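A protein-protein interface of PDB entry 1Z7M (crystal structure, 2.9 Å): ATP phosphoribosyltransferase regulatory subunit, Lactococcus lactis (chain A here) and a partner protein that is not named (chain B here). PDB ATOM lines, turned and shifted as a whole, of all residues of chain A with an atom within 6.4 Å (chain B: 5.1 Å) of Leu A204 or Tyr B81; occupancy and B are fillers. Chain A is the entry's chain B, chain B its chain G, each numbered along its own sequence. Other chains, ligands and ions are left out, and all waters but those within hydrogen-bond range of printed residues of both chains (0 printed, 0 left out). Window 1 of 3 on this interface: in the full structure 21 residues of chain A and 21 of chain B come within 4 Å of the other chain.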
ATOM      1  N   ASN A  75      30.839 -10.870 -10.439  1.00  0.00           N
ATOM      2  CA  ASN A  75      30.943 -10.898 -11.931  1.00  0.00           C
ATOM      3  C   ASN A  75      29.766 -10.655 -12.887  1.00  0.00           C
ATOM      4  O   ASN A  75      29.740  -9.657 -13.595  1.00  0.00           O
ATOM      5  CB  ASN A  75      31.378 -12.284 -12.411  1.00  0.00           C
ATOM      6  CG  ASN A  75      30.792 -12.643 -13.763  1.00  0.00           C
ATOM      7  OD1 ASN A  75      29.999 -11.889 -14.327  1.00  0.00           O
ATOM      8  ND2 ASN A  75      31.198 -13.789 -14.297  1.00  0.00           N
ATOM      9  N   LEU A 199      37.953 -16.144 -19.447  1.00  0.00           N
ATOM     10  CA  LEU A 199      37.094 -17.254 -19.836  1.00  0.00           C
ATOM     11  C   LEU A 199      35.624 -16.967 -19.585  1.00  0.00           C
ATOM     12  O   LEU A 199      34.751 -17.513 -20.253  1.00  0.00           O
ATOM     13  CB  LEU A 199      37.498 -18.509 -19.074  1.00  0.00           C
ATOM     14  CG  LEU A 199      36.966 -19.821 -19.641  1.00  0.00           C
ATOM     15  CD1 LEU A 199      37.473 -20.000 -21.064  1.00  0.00           C
ATOM     16  CD2 LEU A 199      37.427 -20.972 -18.776  1.00  0.00           C
ATOM     17  N   THR A 200      35.349 -16.120 -18.605  1.00  0.00           N
ATOM     18  CA  THR A 200      33.976 -15.769 -18.299  1.00  0.00           C
ATOM     19  C   THR A 200      33.393 -14.957 -19.447  1.00  0.00           C
ATOM     20  O   THR A 200      32.272 -15.195 -19.885  1.00  0.00           O
ATOM     21  CB  THR A 200      33.875 -14.930 -17.023  1.00  0.00           C
ATOM     22  OG1 THR A 200      34.343 -15.690 -15.903  1.00  0.00           O
ATOM     23  CG2 THR A 200      32.439 -14.524 -16.785  1.00  0.00           C
ATOM     24  N   GLU A 201      34.146 -13.987 -19.938  1.00  0.00           N
ATOM     25  CA  GLU A 201      33.640 -13.184 -21.025  1.00  0.00           C
ATOM     26  C   GLU A 201      33.519 -14.034 -22.296  1.00  0.00           C
ATOM     27  O   GLU A 201      32.584 -13.858 -23.085  1.00  0.00           O
ATOM     28  CB  GLU A 201      34.553 -11.982 -21.258  1.00  0.00           C
ATOM     29  CG  GLU A 201      34.051 -11.049 -22.362  1.00  0.00           C
ATOM     30  CD  GLU A 201      32.691 -10.410 -22.039  1.00  0.00           C
ATOM     31  OE1 GLU A 201      32.061  -9.837 -22.967  1.00  0.00           O
ATOM     32  OE2 GLU A 201      32.261 -10.475 -20.858  1.00  0.00           O
ATOM     33  N   LEU A 202      34.454 -14.963 -22.484  1.00  0.00           N
ATOM     34  CA  LEU A 202      34.443 -15.823 -23.656  1.00  0.00           C
ATOM     35  C   LEU A 202      33.229 -16.734 -23.678  1.00  0.00           C
ATOM     36  O   LEU A 202      32.618 -16.940 -24.726  1.00  0.00           O
ATOM     37  CB  LEU A 202      35.726 -16.654 -23.718  1.00  0.00           C
ATOM     38  CG  LEU A 202      36.989 -15.921 -24.193  1.00  0.00           C
ATOM     39  CD1 LEU A 202      38.166 -16.865 -24.179  1.00  0.00           C
ATOM     40  CD2 LEU A 202      36.781 -15.392 -25.593  1.00  0.00           C
ATOM     41  N   LEU A 203      32.874 -17.275 -22.520  1.00  0.00           N
ATOM     42  CA  LEU A 203      31.725 -18.165 -22.403  1.00  0.00           C
ATOM     43  C   LEU A 203      30.394 -17.432 -22.497  1.00  0.00           C
ATOM     44  O   LEU A 203      29.407 -17.966 -23.019  1.00  0.00           O
ATOM     45  CB  LEU A 203      31.790 -18.909 -21.081  1.00  0.00           C
ATOM     46  CG  LEU A 203      32.737 -20.105 -20.994  1.00  0.00           C
ATOM     47  CD1 LEU A 203      32.934 -20.463 -19.545  1.00  0.00           C
ATOM     48  CD2 LEU A 203      32.162 -21.292 -21.750  1.00  0.00           C
ATOM     49  N   LEU A 204      30.376 -16.214 -21.970  1.00  0.00           N
ATOM     50  CA  LEU A 204      29.194 -15.377 -21.974  1.00  0.00           C
ATOM     51  C   LEU A 204      28.739 -15.006 -23.348  1.00  0.00           C
ATOM     52  O   LEU A 204      27.543 -14.978 -23.632  1.00  0.00           O
ATOM     53  CB  LEU A 204      29.470 -14.093 -21.242  1.00  0.00           C
ATOM     54  CG  LEU A 204      29.318 -14.195 -19.744  1.00  0.00           C
ATOM     55  CD1 LEU A 204      29.821 -12.918 -19.108  1.00  0.00           C
ATOM     56  CD2 LEU A 204      27.868 -14.439 -19.422  1.00  0.00           C
ATOM     57  N   LYS A 205      29.709 -14.679 -24.183  1.00  0.00           N
ATOM     58  CA  LYS A 205      29.434 -14.268 -25.535  1.00  0.00           C
ATOM     59  C   LYS A 205      29.645 -15.425 -26.485  1.00  0.00           C
ATOM     60  O   LYS A 205      29.468 -15.272 -27.688  1.00  0.00           O
ATOM     61  CB  LYS A 205      30.369 -13.124 -25.886  1.00  0.00           C
ATOM     62  CG  LYS A 205      30.463 -12.057 -24.803  1.00  0.00           C
ATOM     63  CD  LYS A 205      29.209 -11.196 -24.727  1.00  0.00           C
ATOM     64  CE  LYS A 205      28.868 -10.605 -26.080  1.00  0.00           C
ATOM     65  NZ  LYS A 205      30.029  -9.908 -26.730  1.00  0.00           N
ATOM     66  N   LYS A 206      29.987 -16.590 -25.941  1.00  0.00           N
ATOM     67  CA  LYS A 206      30.246 -17.733 -26.783  1.00  0.00           C
ATOM     68  C   LYS A 206      31.110 -17.237 -27.906  1.00  0.00           C
ATOM     69  O   LYS A 206      30.884 -17.465 -29.102  1.00  0.00           O
ATOM     70  CB  LYS A 206      28.961 -18.376 -27.285  1.00  0.00           C
ATOM     71  CG  LYS A 206      28.164 -19.039 -26.175  1.00  0.00           C
ATOM     72  CD  LYS A 206      27.133 -20.003 -26.726  1.00  0.00           C
ATOM     73  CE  LYS A 206      26.346 -20.657 -25.610  1.00  0.00           C
ATOM     74  NZ  LYS A 206      27.239 -21.209 -24.560  1.00  0.00           N
ATOM     75  N   ASP A 207      32.098 -16.511 -27.448  1.00  0.00           N
ATOM     76  CA  ASP A 207      33.072 -15.885 -28.284  1.00  0.00           C
ATOM     77  C   ASP A 207      34.009 -16.990 -28.912  1.00  0.00           C
ATOM     78  O   ASP A 207      35.193 -17.038 -28.579  1.00  0.00           O
ATOM     79  CB  ASP A 207      33.860 -14.838 -27.496  1.00  0.00           C
ATOM     80  CG  ASP A 207      34.736 -13.977 -28.386  1.00  0.00           C
ATOM     81  OD1 ASP A 207      35.034 -14.407 -29.520  1.00  0.00           O
ATOM     82  OD2 ASP A 207      35.125 -12.874 -27.949  1.00  0.00           O
ATOM     83  N   PHE A 232      31.101 -25.107 -25.551  1.00  0.00           N
ATOM     84  CA  PHE A 232      30.568 -23.846 -26.037  1.00  0.00           C
ATOM     85  C   PHE A 232      29.390 -24.057 -26.965  1.00  0.00           C
ATOM     86  O   PHE A 232      28.579 -23.160 -27.116  1.00  0.00           O
ATOM     87  CB  PHE A 232      31.620 -23.082 -26.832  1.00  0.00           C
ATOM     88  CG  PHE A 232      32.417 -22.098 -26.034  1.00  0.00           C
ATOM     89  CD1 PHE A 232      33.094 -22.488 -24.885  1.00  0.00           C
ATOM     90  CD2 PHE A 232      32.554 -20.792 -26.483  1.00  0.00           C
ATOM     91  CE1 PHE A 232      33.896 -21.590 -24.204  1.00  0.00           C
ATOM     92  CE2 PHE A 232      33.352 -19.893 -25.806  1.00  0.00           C
ATOM     93  CZ  PHE A 232      34.024 -20.290 -24.668  1.00  0.00           C
ATOM     94  N   GLY A 277      28.799 -25.001 -20.331  1.00  0.00           N
ATOM     95  CA  GLY A 277      29.340 -23.709 -20.700  1.00  0.00           C
ATOM     96  C   GLY A 277      28.581 -22.583 -20.035  1.00  0.00           C
ATOM     97  O   GLY A 277      28.736 -21.422 -20.393  1.00  0.00           O
ATOM     98  N   VAL A 279      27.733 -19.839 -17.425  1.00  0.00           N
ATOM     99  CA  VAL A 279      28.503 -18.966 -16.527  1.00  0.00           C
ATOM    100  C   VAL A 279      27.620 -18.581 -15.334  1.00  0.00           C
ATOM    101  O   VAL A 279      26.554 -17.992 -15.506  1.00  0.00           O
ATOM    102  CB  VAL A 279      28.937 -17.667 -17.231  1.00  0.00           C
ATOM    103  CG1 VAL A 279      29.675 -16.811 -16.272  1.00  0.00           C
ATOM    104  CG2 VAL A 279      29.799 -17.961 -18.421  1.00  0.00           C
ATOM    105  N   LEU B  58      17.748  -7.243 -33.219  1.00  0.00           N
ATOM    106  CA  LEU B  58      18.245  -8.455 -32.599  1.00  0.00           C
ATOM    107  C   LEU B  58      17.717  -8.514 -31.177  1.00  0.00           C
ATOM    108  O   LEU B  58      17.179  -9.529 -30.741  1.00  0.00           O
ATOM    109  CB  LEU B  58      19.770  -8.460 -32.570  1.00  0.00           C
ATOM    110  CG  LEU B  58      20.352  -9.801 -32.130  1.00  0.00           C
ATOM    111  CD1 LEU B  58      20.552 -10.678 -33.345  1.00  0.00           C
ATOM    112  CD2 LEU B  58      21.659  -9.588 -31.418  1.00  0.00           C
ATOM    113  N   LEU B  73      29.118  -2.304 -30.933  1.00  0.00           N
ATOM    114  CA  LEU B  73      28.837  -3.171 -29.797  1.00  0.00           C
ATOM    115  C   LEU B  73      29.505  -2.601 -28.568  1.00  0.00           C
ATOM    116  O   LEU B  73      29.033  -2.790 -27.457  1.00  0.00           O
ATOM    117  CB  LEU B  73      29.355  -4.589 -30.039  1.00  0.00           C
ATOM    118  CG  LEU B  73      28.726  -5.478 -31.115  1.00  0.00           C
ATOM    119  CD1 LEU B  73      29.675  -6.624 -31.356  1.00  0.00           C
ATOM    120  CD2 LEU B  73      27.353  -5.996 -30.713  1.00  0.00           C
ATOM    121  N   PHE B  78      23.399  -2.765 -25.212  1.00  0.00           N
ATOM    122  CA  PHE B  78      22.791  -4.088 -25.267  1.00  0.00           C
ATOM    123  C   PHE B  78      23.882  -5.127 -25.069  1.00  0.00           C
ATOM    124  O   PHE B  78      25.012  -4.946 -25.528  1.00  0.00           O
ATOM    125  CB  PHE B  78      22.088  -4.307 -26.600  1.00  0.00           C
ATOM    126  CG  PHE B  78      21.462  -5.664 -26.729  1.00  0.00           C
ATOM    127  CD1 PHE B  78      20.579  -6.137 -25.759  1.00  0.00           C
ATOM    128  CD2 PHE B  78      21.767  -6.484 -27.810  1.00  0.00           C
ATOM    129  CE1 PHE B  78      20.013  -7.403 -25.864  1.00  0.00           C
ATOM    130  CE2 PHE B  78      21.207  -7.754 -27.924  1.00  0.00           C
ATOM    131  CZ  PHE B  78      20.329  -8.212 -26.946  1.00  0.00           C
ATOM    132  N   ASP B  79      23.545  -6.230 -24.411  1.00  0.00           N
ATOM    133  CA  ASP B  79      24.555  -7.230 -24.112  1.00  0.00           C
ATOM    134  C   ASP B  79      24.043  -8.671 -24.019  1.00  0.00           C
ATOM    135  O   ASP B  79      24.749  -9.561 -23.539  1.00  0.00           O
ATOM    136  CB  ASP B  79      25.211  -6.827 -22.794  1.00  0.00           C
ATOM    137  CG  ASP B  79      26.595  -7.396 -22.623  1.00  0.00           C
ATOM    138  OD1 ASP B  79      27.173  -7.169 -21.534  1.00  0.00           O
ATOM    139  OD2 ASP B  79      27.108  -8.061 -23.558  1.00  0.00           O
ATOM    140  N   ASP B  80      22.823  -8.913 -24.478  1.00  0.00           N
ATOM    141  CA  ASP B  80      22.264 -10.261 -24.422  1.00  0.00           C
ATOM    142  C   ASP B  80      22.390 -11.020 -25.725  1.00  0.00           C
ATOM    143  O   ASP B  80      21.395 -11.446 -26.325  1.00  0.00           O
ATOM    144  CB  ASP B  80      20.803 -10.201 -24.012  1.00  0.00           C
ATOM    145  CG  ASP B  80      20.643 -10.210 -22.539  1.00  0.00           C
ATOM    146  OD1 ASP B  80      19.530  -9.938 -22.042  1.00  0.00           O
ATOM    147  OD2 ASP B  80      21.659 -10.498 -21.875  1.00  0.00           O
ATOM    148  N   TYR B  81      23.623 -11.197 -26.165  1.00  0.00           N
ATOM    149  CA  TYR B  81      23.862 -11.902 -27.393  1.00  0.00           C
ATOM    150  C   TYR B  81      25.076 -12.781 -27.231  1.00  0.00           C
ATOM    151  O   TYR B  81      25.642 -12.890 -26.142  1.00  0.00           O
ATOM    152  CB  TYR B  81      24.057 -10.898 -28.540  1.00  0.00           C
ATOM    153  CG  TYR B  81      25.168  -9.884 -28.327  1.00  0.00           C
ATOM    154  CD1 TYR B  81      26.479 -10.159 -28.704  1.00  0.00           C
ATOM    155  CD2 TYR B  81      24.904  -8.650 -27.741  1.00  0.00           C
ATOM    156  CE1 TYR B  81      27.493  -9.227 -28.505  1.00  0.00           C
ATOM    157  CE2 TYR B  81      25.911  -7.717 -27.533  1.00  0.00           C
ATOM    158  CZ  TYR B  81      27.200  -8.008 -27.915  1.00  0.00           C
ATOM    159  OH  TYR B  81      28.190  -7.071 -27.701  1.00  0.00           O
ATOM    160  N   TYR B  82      25.442 -13.432 -28.327  1.00  0.00           N
ATOM    161  CA  TYR B  82      26.604 -14.289 -28.394  1.00  0.00           C
ATOM    162  C   TYR B  82      27.391 -13.706 -29.549  1.00  0.00           C
ATOM    163  O   TYR B  82      26.811 -13.242 -30.529  1.00  0.00           O
ATOM    164  CB  TYR B  82      26.191 -15.721 -28.707  1.00  0.00           C
ATOM    165  CG  TYR B  82      25.511 -16.436 -27.557  1.00  0.00           C
ATOM    166  CD1 TYR B  82      24.509 -17.387 -27.786  1.00  0.00           C
ATOM    167  CD2 TYR B  82      25.881 -16.186 -26.236  1.00  0.00           C
ATOM    168  CE1 TYR B  82      23.892 -18.072 -26.724  1.00  0.00           C
ATOM    169  CE2 TYR B  82      25.274 -16.867 -25.173  1.00  0.00           C
ATOM    170  CZ  TYR B  82      24.287 -17.805 -25.425  1.00  0.00           C
ATOM    171  OH  TYR B  82      23.728 -18.488 -24.372  1.00  0.00           O
ATOM    172  N   GLU B  83      28.707 -13.677 -29.408  1.00  0.00           N
ATOM    173  CA  GLU B  83      29.570 -13.172 -30.462  1.00  0.00           C
ATOM    174  C   GLU B  83      30.203 -14.446 -31.012  1.00  0.00           C
ATOM    175  O   GLU B  83      31.304 -14.832 -30.616  1.00  0.00           O
ATOM    176  CB  GLU B  83      30.630 -12.237 -29.879  1.00  0.00           C
ATOM    177  CG  GLU B  83      31.070 -11.120 -30.820  1.00  0.00           C
ATOM    178  CD  GLU B  83      31.930 -10.068 -30.117  1.00  0.00           C
ATOM    179  OE1 GLU B  83      33.109 -10.377 -29.803  1.00  0.00           O
ATOM    180  OE2 GLU B  83      31.428  -8.936 -29.865  1.00  0.00           O
ATOM    181  N   ILE B 182      26.888 -11.357 -34.380  1.00  0.00           N
ATOM    182  CA  ILE B 182      26.240 -11.575 -33.089  1.00  0.00           C
ATOM    183  C   ILE B 182      24.962 -12.398 -33.228  1.00  0.00           C
ATOM    184  O   ILE B 182      24.320 -12.413 -34.276  1.00  0.00           O
ATOM    185  CB  ILE B 182      25.927 -10.230 -32.403  1.00  0.00           C
ATOM    186  CG1 ILE B 182      24.937  -9.421 -33.243  1.00  0.00           C
ATOM    187  CG2 ILE B 182      27.213  -9.418 -32.244  1.00  0.00           C
ATOM    188  CD1 ILE B 182      24.570  -8.087 -32.629  1.00  0.00           C
ATOM    189  N   VAL B 183      24.571 -13.067 -32.159  1.00  0.00           N
ATOM    190  CA  VAL B 183      23.405 -13.921 -32.244  1.00  0.00           C
ATOM    191  C   VAL B 183      22.467 -13.816 -31.052  1.00  0.00           C
ATOM    192  O   VAL B 183      22.886 -13.561 -29.927  1.00  0.00           O
ATOM    193  CB  VAL B 183      23.860 -15.381 -32.435  1.00  0.00           C
ATOM    194  CG1 VAL B 183      22.712 -16.338 -32.236  1.00  0.00           C
ATOM    195  CG2 VAL B 183      24.451 -15.539 -33.818  1.00  0.00           C
ATOM    196  N   ASN B 184      21.185 -14.010 -31.315  1.00  0.00           N
ATOM    197  CA  ASN B 184      20.182 -13.936 -30.279  1.00  0.00           C
ATOM    198  C   ASN B 184      20.299 -15.159 -29.413  1.00  0.00           C
ATOM    199  O   ASN B 184      20.168 -16.273 -29.900  1.00  0.00           O
ATOM    200  CB  ASN B 184      18.804 -13.886 -30.912  1.00  0.00           C
ATOM    201  CG  ASN B 184      17.702 -13.729 -29.897  1.00  0.00           C
ATOM    202  OD1 ASN B 184      17.404 -14.652 -29.113  1.00  0.00           O
ATOM    203  ND2 ASN B 184      17.081 -12.548 -29.895  1.00  0.00           N
ATOM    204  N   LYS B 185      20.557 -14.946 -28.130  1.00  0.00           N
ATOM    205  CA  LYS B 185      20.698 -16.049 -27.181  1.00  0.00           C
ATOM    206  C   LYS B 185      19.549 -17.060 -27.294  1.00  0.00           C
ATOM    207  O   LYS B 185      19.754 -18.270 -27.158  1.00  0.00           O
ATOM    208  CB  LYS B 185      20.754 -15.514 -25.739  1.00  0.00           C
ATOM    209  CG  LYS B 185      22.030 -14.765 -25.345  1.00  0.00           C
ATOM    210  CD  LYS B 185      22.042 -14.467 -23.851  1.00  0.00           C
ATOM    211  CE  LYS B 185      23.221 -13.569 -23.495  1.00  0.00           C
ATOM    212  NZ  LYS B 185      23.242 -13.081 -22.076  1.00  0.00           N
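Thr A200 touches none of the printed residues of chain B.
Leu A202 touches none of the printed residues of chain B.
Of the printed residues of chain B, Lys A206 touches Tyr B82 (3.5 Å) and Glu B83 (3.1 Å).
Printed residues of chain B within 4 Å of Asp A207: Glu B83.
Tyr B81 touches just these residues of chain A: Leu A204 and Lys A205.
The nearest residue of chain A that does not touch Tyr B81 is Lys A206 (5.7 Å).
The nearest printed residue of chain B that does not touch Lys A206 is Tyr B81 (5.7 Å).
O of Glu B83 sits close to O of Lys A206, at 3.1 Å.
NZ of Lys A205 is in salt-bridge range of OE2 of Glu B83 (3.6 Å).
The backbone carbonyl oxygen of Tyr B82 lies within hydrogen-bond range of the backbone NH of Val B183 (2.8 Å).
NZ of Lys A206 is in hydrogen-bond range of O of Phe A232 (3.5 Å).
O of Leu A202 sits at hydrogen-bond distance from N of Asp A207 (2.8 Å).
Printed residues of chain B that touch a printed residue of chain A: Asp B79, Tyr B81, Tyr B82 and Glu B83.
Hydrophobic or aromatic side chains of chain B that line the printed part of chain A: Tyr B81 and Tyr B82.
Among the printed residues, Asp or Glu carboxylates within 4 Å of a Lys or Arg side-chain nitrogen of the other chain: Lys A205 with Glu B83.
Among the printed residues, merely in contact across the chains: Leu A204 with Tyr B81 (3.8 Å), Leu A204 with Tyr B82 (3.3 Å), Lys A205 with Asp B79 (3.95 Å), Lys A205 with Tyr B81 (3.1 Å), Lys A205 with Tyr B82 (3.1 Å), Lys A206 with Tyr B82 (3.5 Å) and Asp A207 with Glu B83 (3.1 Å).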
